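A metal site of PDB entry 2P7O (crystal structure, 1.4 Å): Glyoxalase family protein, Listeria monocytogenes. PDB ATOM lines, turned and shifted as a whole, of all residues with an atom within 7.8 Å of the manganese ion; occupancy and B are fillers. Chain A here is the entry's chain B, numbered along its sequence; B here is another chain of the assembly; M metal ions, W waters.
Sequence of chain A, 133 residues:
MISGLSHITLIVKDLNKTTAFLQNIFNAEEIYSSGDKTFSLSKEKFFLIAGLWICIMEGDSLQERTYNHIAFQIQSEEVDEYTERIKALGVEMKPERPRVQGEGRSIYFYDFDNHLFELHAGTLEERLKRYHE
A ring nitrogen (ND1) of His 120 sits at hydrogen-bond distance from the side-chain carboxylate of Glu 118, 3.2 Å away.
OE2 of Glu 118 lies within hydrogen-bond range of OG of Ser 106 (2.6 Å).
OG of Ser 6 of chain B is in hydrogen-bond range of ND1 of His 7 of chain B (2.7 Å).
The side-chain hydroxyl of Tyr 108 is in hydrogen-bond range of the side-chain carboxylate of Glu 126.
OG1 of Thr 9 of chain B sits close to OE1 of Glu 126.
The backbone NH (N) of Thr 9 of chain B sits at hydrogen-bond distance from the backbone carbonyl oxygen (O) of His 69 (3.0 Å).
ND1 of His 69 is in hydrogen-bond range of O of Tyr 67 (2.8 Å).
The backbone NH (N) of Leu 128 is in hydrogen-bond range of the side-chain hydroxyl (OH) of Tyr 108, 3.1 Å away.
Residues that only touch the manganese ion: Tyr 108 (3.4 Å) and Thr 9 of chain B (3.8 Å).
The nearest printed residue that does not touch the manganese ion is Glu 125 (4.4 Å).
The manganese ion is bound by OE1 of Glu 118 (2.0 Å).
A ring nitrogen (NE2) of His 7 of chain B is bound to the manganese ion, at 2.2 Å.
The manganese ion is bound by OE1 of Glu 126, at 2.2 Å.
The manganese ion is bound by water W1, at 2.3 Å.
The manganese ion is bound by NE2 of His 69, at 2.3 Å.
The manganese ion has five donor atoms within binding distance.
Water W1 lies within hydrogen-bond range of OE2 of Glu 118, O of Glu 125, N of Arg 127, OH of Tyr 108 and ND1 of His 120.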
ATOM      1  N   TYR A  67     -18.182  17.703  18.388  1.00  0.00           N
ATOM      2  CA  TYR A  67     -19.343  17.974  17.561  1.00  0.00           C
ATOM      3  C   TYR A  67     -20.320  18.913  18.277  1.00  0.00           C
ATOM      4  O   TYR A  67     -21.322  19.284  17.614  1.00  0.00           O
ATOM      5  CB  TYR A  67     -20.065  16.688  17.157  1.00  0.00           C
ATOM      6  CG  TYR A  67     -19.552  15.961  15.945  1.00  0.00           C
ATOM      7  CD1 TYR A  67     -20.130  14.752  15.555  1.00  0.00           C
ATOM      8  CD2 TYR A  67     -18.533  16.497  15.181  1.00  0.00           C
ATOM      9  CE1 TYR A  67     -19.685  14.051  14.441  1.00  0.00           C
ATOM     10  CE2 TYR A  67     -18.091  15.824  14.057  1.00  0.00           C
ATOM     11  CZ  TYR A  67     -18.668  14.616  13.698  1.00  0.00           C
ATOM     12  OH  TYR A  67     -18.167  14.025  12.544  1.00  0.00           O
ATOM     13  N   HIS A  69     -21.804  22.507  18.859  1.00  0.00           N
ATOM     14  CA  HIS A  69     -21.647  23.642  17.932  1.00  0.00           C
ATOM     15  C   HIS A  69     -22.775  24.625  18.135  1.00  0.00           C
ATOM     16  O   HIS A  69     -23.849  24.283  18.651  1.00  0.00           O
ATOM     17  CB  HIS A  69     -21.617  23.178  16.494  1.00  0.00           C
ATOM     18  CG  HIS A  69     -22.751  22.362  15.969  1.00  0.00           C
ATOM     19  ND1 HIS A  69     -22.891  21.009  16.156  1.00  0.00           N
ATOM     20  CD2 HIS A  69     -23.809  22.741  15.230  1.00  0.00           C
ATOM     21  CE1 HIS A  69     -23.997  20.608  15.525  1.00  0.00           C
ATOM     22  NE2 HIS A  69     -24.607  21.663  14.986  1.00  0.00           N
ATOM     23  N   ILE A  70     -22.542  25.847  17.697  1.00  0.00           N
ATOM     24  CA  ILE A  70     -23.493  26.939  17.478  1.00  0.00           C
ATOM     25  C   ILE A  70     -23.832  27.036  15.981  1.00  0.00           C
ATOM     26  O   ILE A  70     -22.857  27.166  15.234  1.00  0.00           O
ATOM     27  CB  ILE A  70     -22.858  28.295  17.900  1.00  0.00           C
ATOM     28  CG1 ILE A  70     -22.478  28.189  19.388  1.00  0.00           C
ATOM     29  CG2 ILE A  70     -23.833  29.434  17.706  1.00  0.00           C
ATOM     30  CD1 ILE A  70     -23.739  27.734  20.138  1.00  0.00           C
ATOM     31  N   ALA A  71     -25.114  26.986  15.620  1.00  0.00           N
ATOM     32  CA  ALA A  71     -25.550  27.183  14.228  1.00  0.00           C
ATOM     33  C   ALA A  71     -26.301  28.528  14.138  1.00  0.00           C
ATOM     34  O   ALA A  71     -27.282  28.713  14.869  1.00  0.00           O
ATOM     35  CB  ALA A  71     -26.538  26.105  13.816  1.00  0.00           C
ATOM     36  N   PHE A  72     -25.905  29.294  13.139  1.00  0.00           N
ATOM     37  CA  PHE A  72     -26.529  30.531  12.726  1.00  0.00           C
ATOM     38  C   PHE A  72     -27.355  30.310  11.444  1.00  0.00           C
ATOM     39  O   PHE A  72     -26.947  29.530  10.603  1.00  0.00           O
ATOM     40  CB  PHE A  72     -25.487  31.638  12.479  1.00  0.00           C
ATOM     41  CG  PHE A  72     -24.882  32.144  13.799  1.00  0.00           C
ATOM     42  CD1 PHE A  72     -23.656  31.634  14.201  1.00  0.00           C
ATOM     43  CD2 PHE A  72     -25.511  33.070  14.591  1.00  0.00           C
ATOM     44  CE1 PHE A  72     -23.081  32.080  15.395  1.00  0.00           C
ATOM     45  CE2 PHE A  72     -24.956  33.510  15.776  1.00  0.00           C
ATOM     46  CZ  PHE A  72     -23.714  33.047  16.183  1.00  0.00           C
ATOM     47  N   SER A 106     -26.085  23.044   4.880  1.00  0.00           N
ATOM     48  CA  SER A 106     -25.319  23.703   5.942  1.00  0.00           C
ATOM     49  C   SER A 106     -23.830  23.749   5.612  1.00  0.00           C
ATOM     50  O   SER A 106     -23.365  22.995   4.761  1.00  0.00           O
ATOM     51  CB  SER A 106     -25.401  22.870   7.238  1.00  0.00           C
ATOM     52  OG  SER A 106     -26.672  23.150   7.832  1.00  0.00           O
ATOM     53  N   TYR A 108     -20.265  23.416   7.784  1.00  0.00           N
ATOM     54  CA  TYR A 108     -19.661  23.211   9.093  1.00  0.00           C
ATOM     55  C   TYR A 108     -18.173  23.577   9.063  1.00  0.00           C
ATOM     56  O   TYR A 108     -17.452  23.200   8.128  1.00  0.00           O
ATOM     57  CB  TYR A 108     -19.733  21.767   9.630  1.00  0.00           C
ATOM     58  CG  TYR A 108     -21.086  21.274  10.065  1.00  0.00           C
ATOM     59  CD1 TYR A 108     -22.031  20.832   9.139  1.00  0.00           C
ATOM     60  CD2 TYR A 108     -21.419  21.177  11.419  1.00  0.00           C
ATOM     61  CE1 TYR A 108     -23.265  20.349   9.558  1.00  0.00           C
ATOM     62  CE2 TYR A 108     -22.676  20.723  11.839  1.00  0.00           C
ATOM     63  CZ  TYR A 108     -23.617  20.322  10.877  1.00  0.00           C
ATOM     64  OH  TYR A 108     -24.823  19.838  11.254  1.00  0.00           O
ATOM     65  N   LEU A 116     -16.560  24.471  16.764  1.00  0.00           N
ATOM     66  CA  LEU A 116     -17.292  24.150  15.528  1.00  0.00           C
ATOM     67  C   LEU A 116     -18.498  25.051  15.410  1.00  0.00           C
ATOM     68  O   LEU A 116     -19.267  25.149  16.360  1.00  0.00           O
ATOM     69  CB  LEU A 116     -17.721  22.688  15.544  1.00  0.00           C
ATOM     70  CG  LEU A 116     -18.572  22.188  14.362  1.00  0.00           C
ATOM     71  CD1 LEU A 116     -17.805  22.119  13.040  1.00  0.00           C
ATOM     72  CD2 LEU A 116     -19.081  20.761  14.653  1.00  0.00           C
ATOM     73  N   PHE A 117     -18.608  25.664  14.227  1.00  0.00           N
ATOM     74  CA  PHE A 117     -19.777  26.523  13.944  1.00  0.00           C
ATOM     75  C   PHE A 117     -20.503  25.908  12.780  1.00  0.00           C
ATOM     76  O   PHE A 117     -19.904  25.213  11.928  1.00  0.00           O
ATOM     77  CB  PHE A 117     -19.239  27.910  13.528  1.00  0.00           C
ATOM     78  CG  PHE A 117     -18.867  28.801  14.693  1.00  0.00           C
ATOM     79  CD1 PHE A 117     -17.595  28.764  15.265  1.00  0.00           C
ATOM     80  CD2 PHE A 117     -19.807  29.631  15.299  1.00  0.00           C
ATOM     81  CE1 PHE A 117     -17.266  29.490  16.405  1.00  0.00           C
ATOM     82  CE2 PHE A 117     -19.491  30.380  16.419  1.00  0.00           C
ATOM     83  CZ  PHE A 117     -18.227  30.330  16.986  1.00  0.00           C
ATOM     84  N   GLU A 118     -21.754  26.301  12.632  1.00  0.00           N
ATOM     85  CA  GLU A 118     -22.561  25.883  11.484  1.00  0.00           C
ATOM     86  C   GLU A 118     -23.299  27.099  10.963  1.00  0.00           C
ATOM     87  O   GLU A 118     -23.832  27.886  11.750  1.00  0.00           O
ATOM     88  CB  GLU A 118     -23.587  24.803  11.891  1.00  0.00           C
ATOM     89  CG  GLU A 118     -24.491  24.257  10.747  1.00  0.00           C
ATOM     90  CD  GLU A 118     -25.510  23.232  11.219  1.00  0.00           C
ATOM     91  OE1 GLU A 118     -25.565  22.936  12.451  1.00  0.00           O
ATOM     92  OE2 GLU A 118     -26.318  22.703  10.418  1.00  0.00           O
ATOM     93  N   LEU A 119     -23.379  27.206   9.641  1.00  0.00           N
ATOM     94  CA  LEU A 119     -24.329  28.109   9.010  1.00  0.00           C
ATOM     95  C   LEU A 119     -25.385  27.219   8.278  1.00  0.00           C
ATOM     96  O   LEU A 119     -24.987  26.365   7.474  1.00  0.00           O
ATOM     97  CB  LEU A 119     -23.667  29.007   7.982  1.00  0.00           C
ATOM     98  CG  LEU A 119     -22.659  29.998   8.595  1.00  0.00           C
ATOM     99  CD1 LEU A 119     -21.999  30.786   7.468  1.00  0.00           C
ATOM    100  CD2 LEU A 119     -23.430  30.986   9.493  1.00  0.00           C
ATOM    101  N   HIS A 120     -26.607  27.434   8.703  1.00  0.00           N
ATOM    102  CA  HIS A 120     -27.687  26.510   8.396  1.00  0.00           C
ATOM    103  C   HIS A 120     -28.756  27.218   7.561  1.00  0.00           C
ATOM    104  O   HIS A 120     -29.379  28.205   8.012  1.00  0.00           O
ATOM    105  CB  HIS A 120     -28.238  26.045   9.789  1.00  0.00           C
ATOM    106  CG  HIS A 120     -29.377  25.072   9.607  1.00  0.00           C
ATOM    107  ND1 HIS A 120     -29.309  23.763  10.020  1.00  0.00           N
ATOM    108  CD2 HIS A 120     -30.680  25.188   9.208  1.00  0.00           C
ATOM    109  CE1 HIS A 120     -30.459  23.142   9.808  1.00  0.00           C
ATOM    110  NE2 HIS A 120     -31.299  23.978   9.221  1.00  0.00           N
ATOM    111  N   LEU A 124     -35.159  23.137   9.903  1.00  0.00           N
ATOM    112  CA  LEU A 124     -34.367  22.908  11.102  1.00  0.00           C
ATOM    113  C   LEU A 124     -34.218  21.433  11.350  1.00  0.00           C
ATOM    114  O   LEU A 124     -35.183  20.693  11.338  1.00  0.00           O
ATOM    115  CB  LEU A 124     -34.945  23.665  12.303  1.00  0.00           C
ATOM    116  CG  LEU A 124     -34.334  23.332  13.668  1.00  0.00           C
ATOM    117  CD1 LEU A 124     -32.852  23.659  13.620  1.00  0.00           C
ATOM    118  CD2 LEU A 124     -35.010  24.184  14.752  1.00  0.00           C
ATOM    119  N   GLU A 125     -32.983  21.033  11.575  1.00  0.00           N
ATOM    120  CA  GLU A 125     -32.622  19.656  11.839  1.00  0.00           C
ATOM    121  C   GLU A 125     -31.125  19.650  12.143  1.00  0.00           C
ATOM    122  O   GLU A 125     -30.348  20.570  11.828  1.00  0.00           O
ATOM    123  CB  GLU A 125     -32.961  18.731  10.654  1.00  0.00           C
ATOM    124  CG  GLU A 125     -32.565  19.348   9.326  1.00  0.00           C
ATOM    125  CD  GLU A 125     -32.805  18.503   8.090  1.00  0.00           C
ATOM    126  OE1 GLU A 125     -33.788  17.725   8.038  1.00  0.00           O
ATOM    127  OE2 GLU A 125     -32.062  18.707   7.096  1.00  0.00           O
ATOM    128  N   GLU A 126     -30.706  18.507  12.685  1.00  0.00           N
ATOM    129  CA  GLU A 126     -29.264  18.321  12.894  1.00  0.00           C
ATOM    130  C   GLU A 126     -28.699  17.522  11.729  1.00  0.00           C
ATOM    131  O   GLU A 126     -29.097  16.360  11.437  1.00  0.00           O
ATOM    132  CB  GLU A 126     -29.063  17.597  14.244  1.00  0.00           C
ATOM    133  CG  GLU A 126     -27.556  17.398  14.511  1.00  0.00           C
ATOM    134  CD  GLU A 126     -26.798  18.679  14.227  1.00  0.00           C
ATOM    135  OE1 GLU A 126     -27.206  19.752  14.719  1.00  0.00           O
ATOM    136  OE2 GLU A 126     -25.792  18.528  13.462  1.00  0.00           O
ATOM    137  N   ARG A 127     -27.711  18.123  11.101  1.00  0.00           N
ATOM    138  CA  ARG A 127     -27.159  17.505   9.882  1.00  0.00           C
ATOM    139  C   ARG A 127     -25.788  16.862  10.064  1.00  0.00           C
ATOM    140  O   ARG A 127     -25.182  16.484   9.046  1.00  0.00           O
ATOM    141  CB  ARG A 127     -27.088  18.625   8.823  1.00  0.00           C
ATOM    142  CG  ARG A 127     -28.510  18.998   8.440  1.00  0.00           C
ATOM    143  CD  ARG A 127     -28.538  20.344   7.695  1.00  0.00           C
ATOM    144  NE  ARG A 127     -29.907  20.661   7.257  1.00  0.00           N
ATOM    145  CZ  ARG A 127     -30.257  21.858   6.781  1.00  0.00           C
ATOM    146  NH1 ARG A 127     -29.355  22.844   6.696  1.00  0.00           N
ATOM    147  NH2 ARG A 127     -31.525  22.098   6.359  1.00  0.00           N
ATOM    148  N   LEU A 128     -25.236  16.802  11.258  1.00  0.00           N
ATOM    149  CA  LEU A 128     -23.852  16.297  11.402  1.00  0.00           C
ATOM    150  C   LEU A 128     -23.714  14.895  10.807  1.00  0.00           C
ATOM    151  O   LEU A 128     -22.691  14.492  10.228  1.00  0.00           O
ATOM    152  CB  LEU A 128     -23.416  16.305  12.860  1.00  0.00           C
ATOM    153  CG  LEU A 128     -22.897  17.564  13.563  1.00  0.00           C
ATOM    154  CD1 LEU A 128     -22.863  17.416  15.091  1.00  0.00           C
ATOM    155  CD2 LEU A 128     -21.500  17.902  13.066  1.00  0.00           C
ATOM    156  N   SER B   6     -29.944  29.679  14.595  1.00  0.00           N
ATOM    157  CA  SER B   6     -30.628  28.482  14.159  1.00  0.00           C
ATOM    158  C   SER B   6     -30.842  27.530  15.350  1.00  0.00           C
ATOM    159  O   SER B   6     -31.989  27.195  15.641  1.00  0.00           O
ATOM    160  CB  SER B   6     -29.806  27.692  13.105  1.00  0.00           C
ATOM    161  OG  SER B   6     -30.527  26.515  12.768  1.00  0.00           O
ATOM    162  N   HIS B   7     -29.737  27.132  15.990  1.00  0.00           N
ATOM    163  CA  HIS B   7     -29.882  26.145  17.087  1.00  0.00           C
ATOM    164  C   HIS B   7     -28.527  26.046  17.755  1.00  0.00           C
ATOM    165  O   HIS B   7     -27.518  26.492  17.192  1.00  0.00           O
ATOM    166  CB  HIS B   7     -30.356  24.761  16.587  1.00  0.00           C
ATOM    167  CG  HIS B   7     -29.484  24.079  15.579  1.00  0.00           C
ATOM    168  ND1 HIS B   7     -29.594  24.437  14.221  1.00  0.00           N
ATOM    169  CD2 HIS B   7     -28.538  23.127  15.621  1.00  0.00           C
ATOM    170  CE1 HIS B   7     -28.752  23.702  13.497  1.00  0.00           C
ATOM    171  NE2 HIS B   7     -28.096  22.903  14.316  1.00  0.00           N
ATOM    172  N   ILE B   8     -28.503  25.362  18.890  1.00  0.00           N
ATOM    173  CA  ILE B   8     -27.225  24.916  19.450  1.00  0.00           C
ATOM    174  C   ILE B   8     -27.327  23.411  19.648  1.00  0.00           C
ATOM    175  O   ILE B   8     -28.403  22.952  20.046  1.00  0.00           O
ATOM    176  CB  ILE B   8     -27.064  25.616  20.791  1.00  0.00           C
ATOM    177  CG1 ILE B   8     -26.944  27.155  20.623  1.00  0.00           C
ATOM    178  CG2 ILE B   8     -25.867  25.091  21.549  1.00  0.00           C
ATOM    179  CD1 ILE B   8     -26.882  27.851  21.988  1.00  0.00           C
ATOM    180  N   THR B   9     -26.291  22.671  19.348  1.00  0.00           N
ATOM    181  CA  THR B   9     -26.312  21.223  19.493  1.00  0.00           C
ATOM    182  C   THR B   9     -25.250  20.856  20.537  1.00  0.00           C
ATOM    183  O   THR B   9     -24.070  21.229  20.401  1.00  0.00           O
ATOM    184  CB  THR B   9     -26.036  20.568  18.121  1.00  0.00           C
ATOM    185  OG1 THR B   9     -27.227  20.763  17.332  1.00  0.00           O
ATOM    186  CG2 THR B   9     -25.691  19.085  18.242  1.00  0.00           C
ATOM    187  N   PHE B  46     -34.729  17.246  20.313  1.00  0.00           N
ATOM    188  CA  PHE B  46     -34.764  18.716  20.309  1.00  0.00           C
ATOM    189  C   PHE B  46     -35.639  19.226  21.464  1.00  0.00           C
ATOM    190  O   PHE B  46     -36.686  18.651  21.797  1.00  0.00           O
ATOM    191  CB  PHE B  46     -35.266  19.253  18.966  1.00  0.00           C
ATOM    192  CG  PHE B  46     -34.198  19.596  17.940  1.00  0.00           C
ATOM    193  CD1 PHE B  46     -33.769  20.899  17.779  1.00  0.00           C
ATOM    194  CD2 PHE B  46     -33.662  18.586  17.127  1.00  0.00           C
ATOM    195  CE1 PHE B  46     -32.818  21.226  16.813  1.00  0.00           C
ATOM    196  CE2 PHE B  46     -32.729  18.904  16.175  1.00  0.00           C
ATOM    197  CZ  PHE B  46     -32.282  20.239  16.034  1.00  0.00           C
ATOM    198  N   CYS B  55     -30.579  21.122  20.361  1.00  0.00           N
ATOM    199  CA  CYS B  55     -30.540  19.673  20.092  1.00  0.00           C
ATOM    200  C   CYS B  55     -29.533  19.014  20.995  1.00  0.00           C
ATOM    201  O   CYS B  55     -28.395  19.551  21.184  1.00  0.00           O
ATOM    202  CB  CYS B  55     -30.073  19.506  18.607  1.00  0.00           C
ATOM    203  SG  CYS B  55     -29.643  17.820  18.184  1.00  0.00           S
ATOM    204  N   MET B  57     -27.540  15.225  21.454  1.00  0.00           N
ATOM    205  CA  MET B  57     -27.153  14.090  20.613  1.00  0.00           C
ATOM    206  C   MET B  57     -26.195  13.191  21.401  1.00  0.00           C
ATOM    207  O   MET B  57     -25.303  13.714  22.065  1.00  0.00           O
ATOM    208  CB  MET B  57     -26.560  14.689  19.342  1.00  0.00           C
ATOM    209  CG  MET B  57     -25.493  14.047  18.497  1.00  0.00           C
ATOM    210  SD  MET B  57     -25.317  14.863  16.845  1.00  0.00           S
ATOM    211  CE  MET B  57     -26.919  14.303  16.192  1.00  0.00           C
HETATM  212 MN    MN M   1     -26.490  21.588  13.664  1.00  0.00          MN
HETATM  213  O   HOH W   1     -27.717  21.240  11.752  1.00  0.00           O
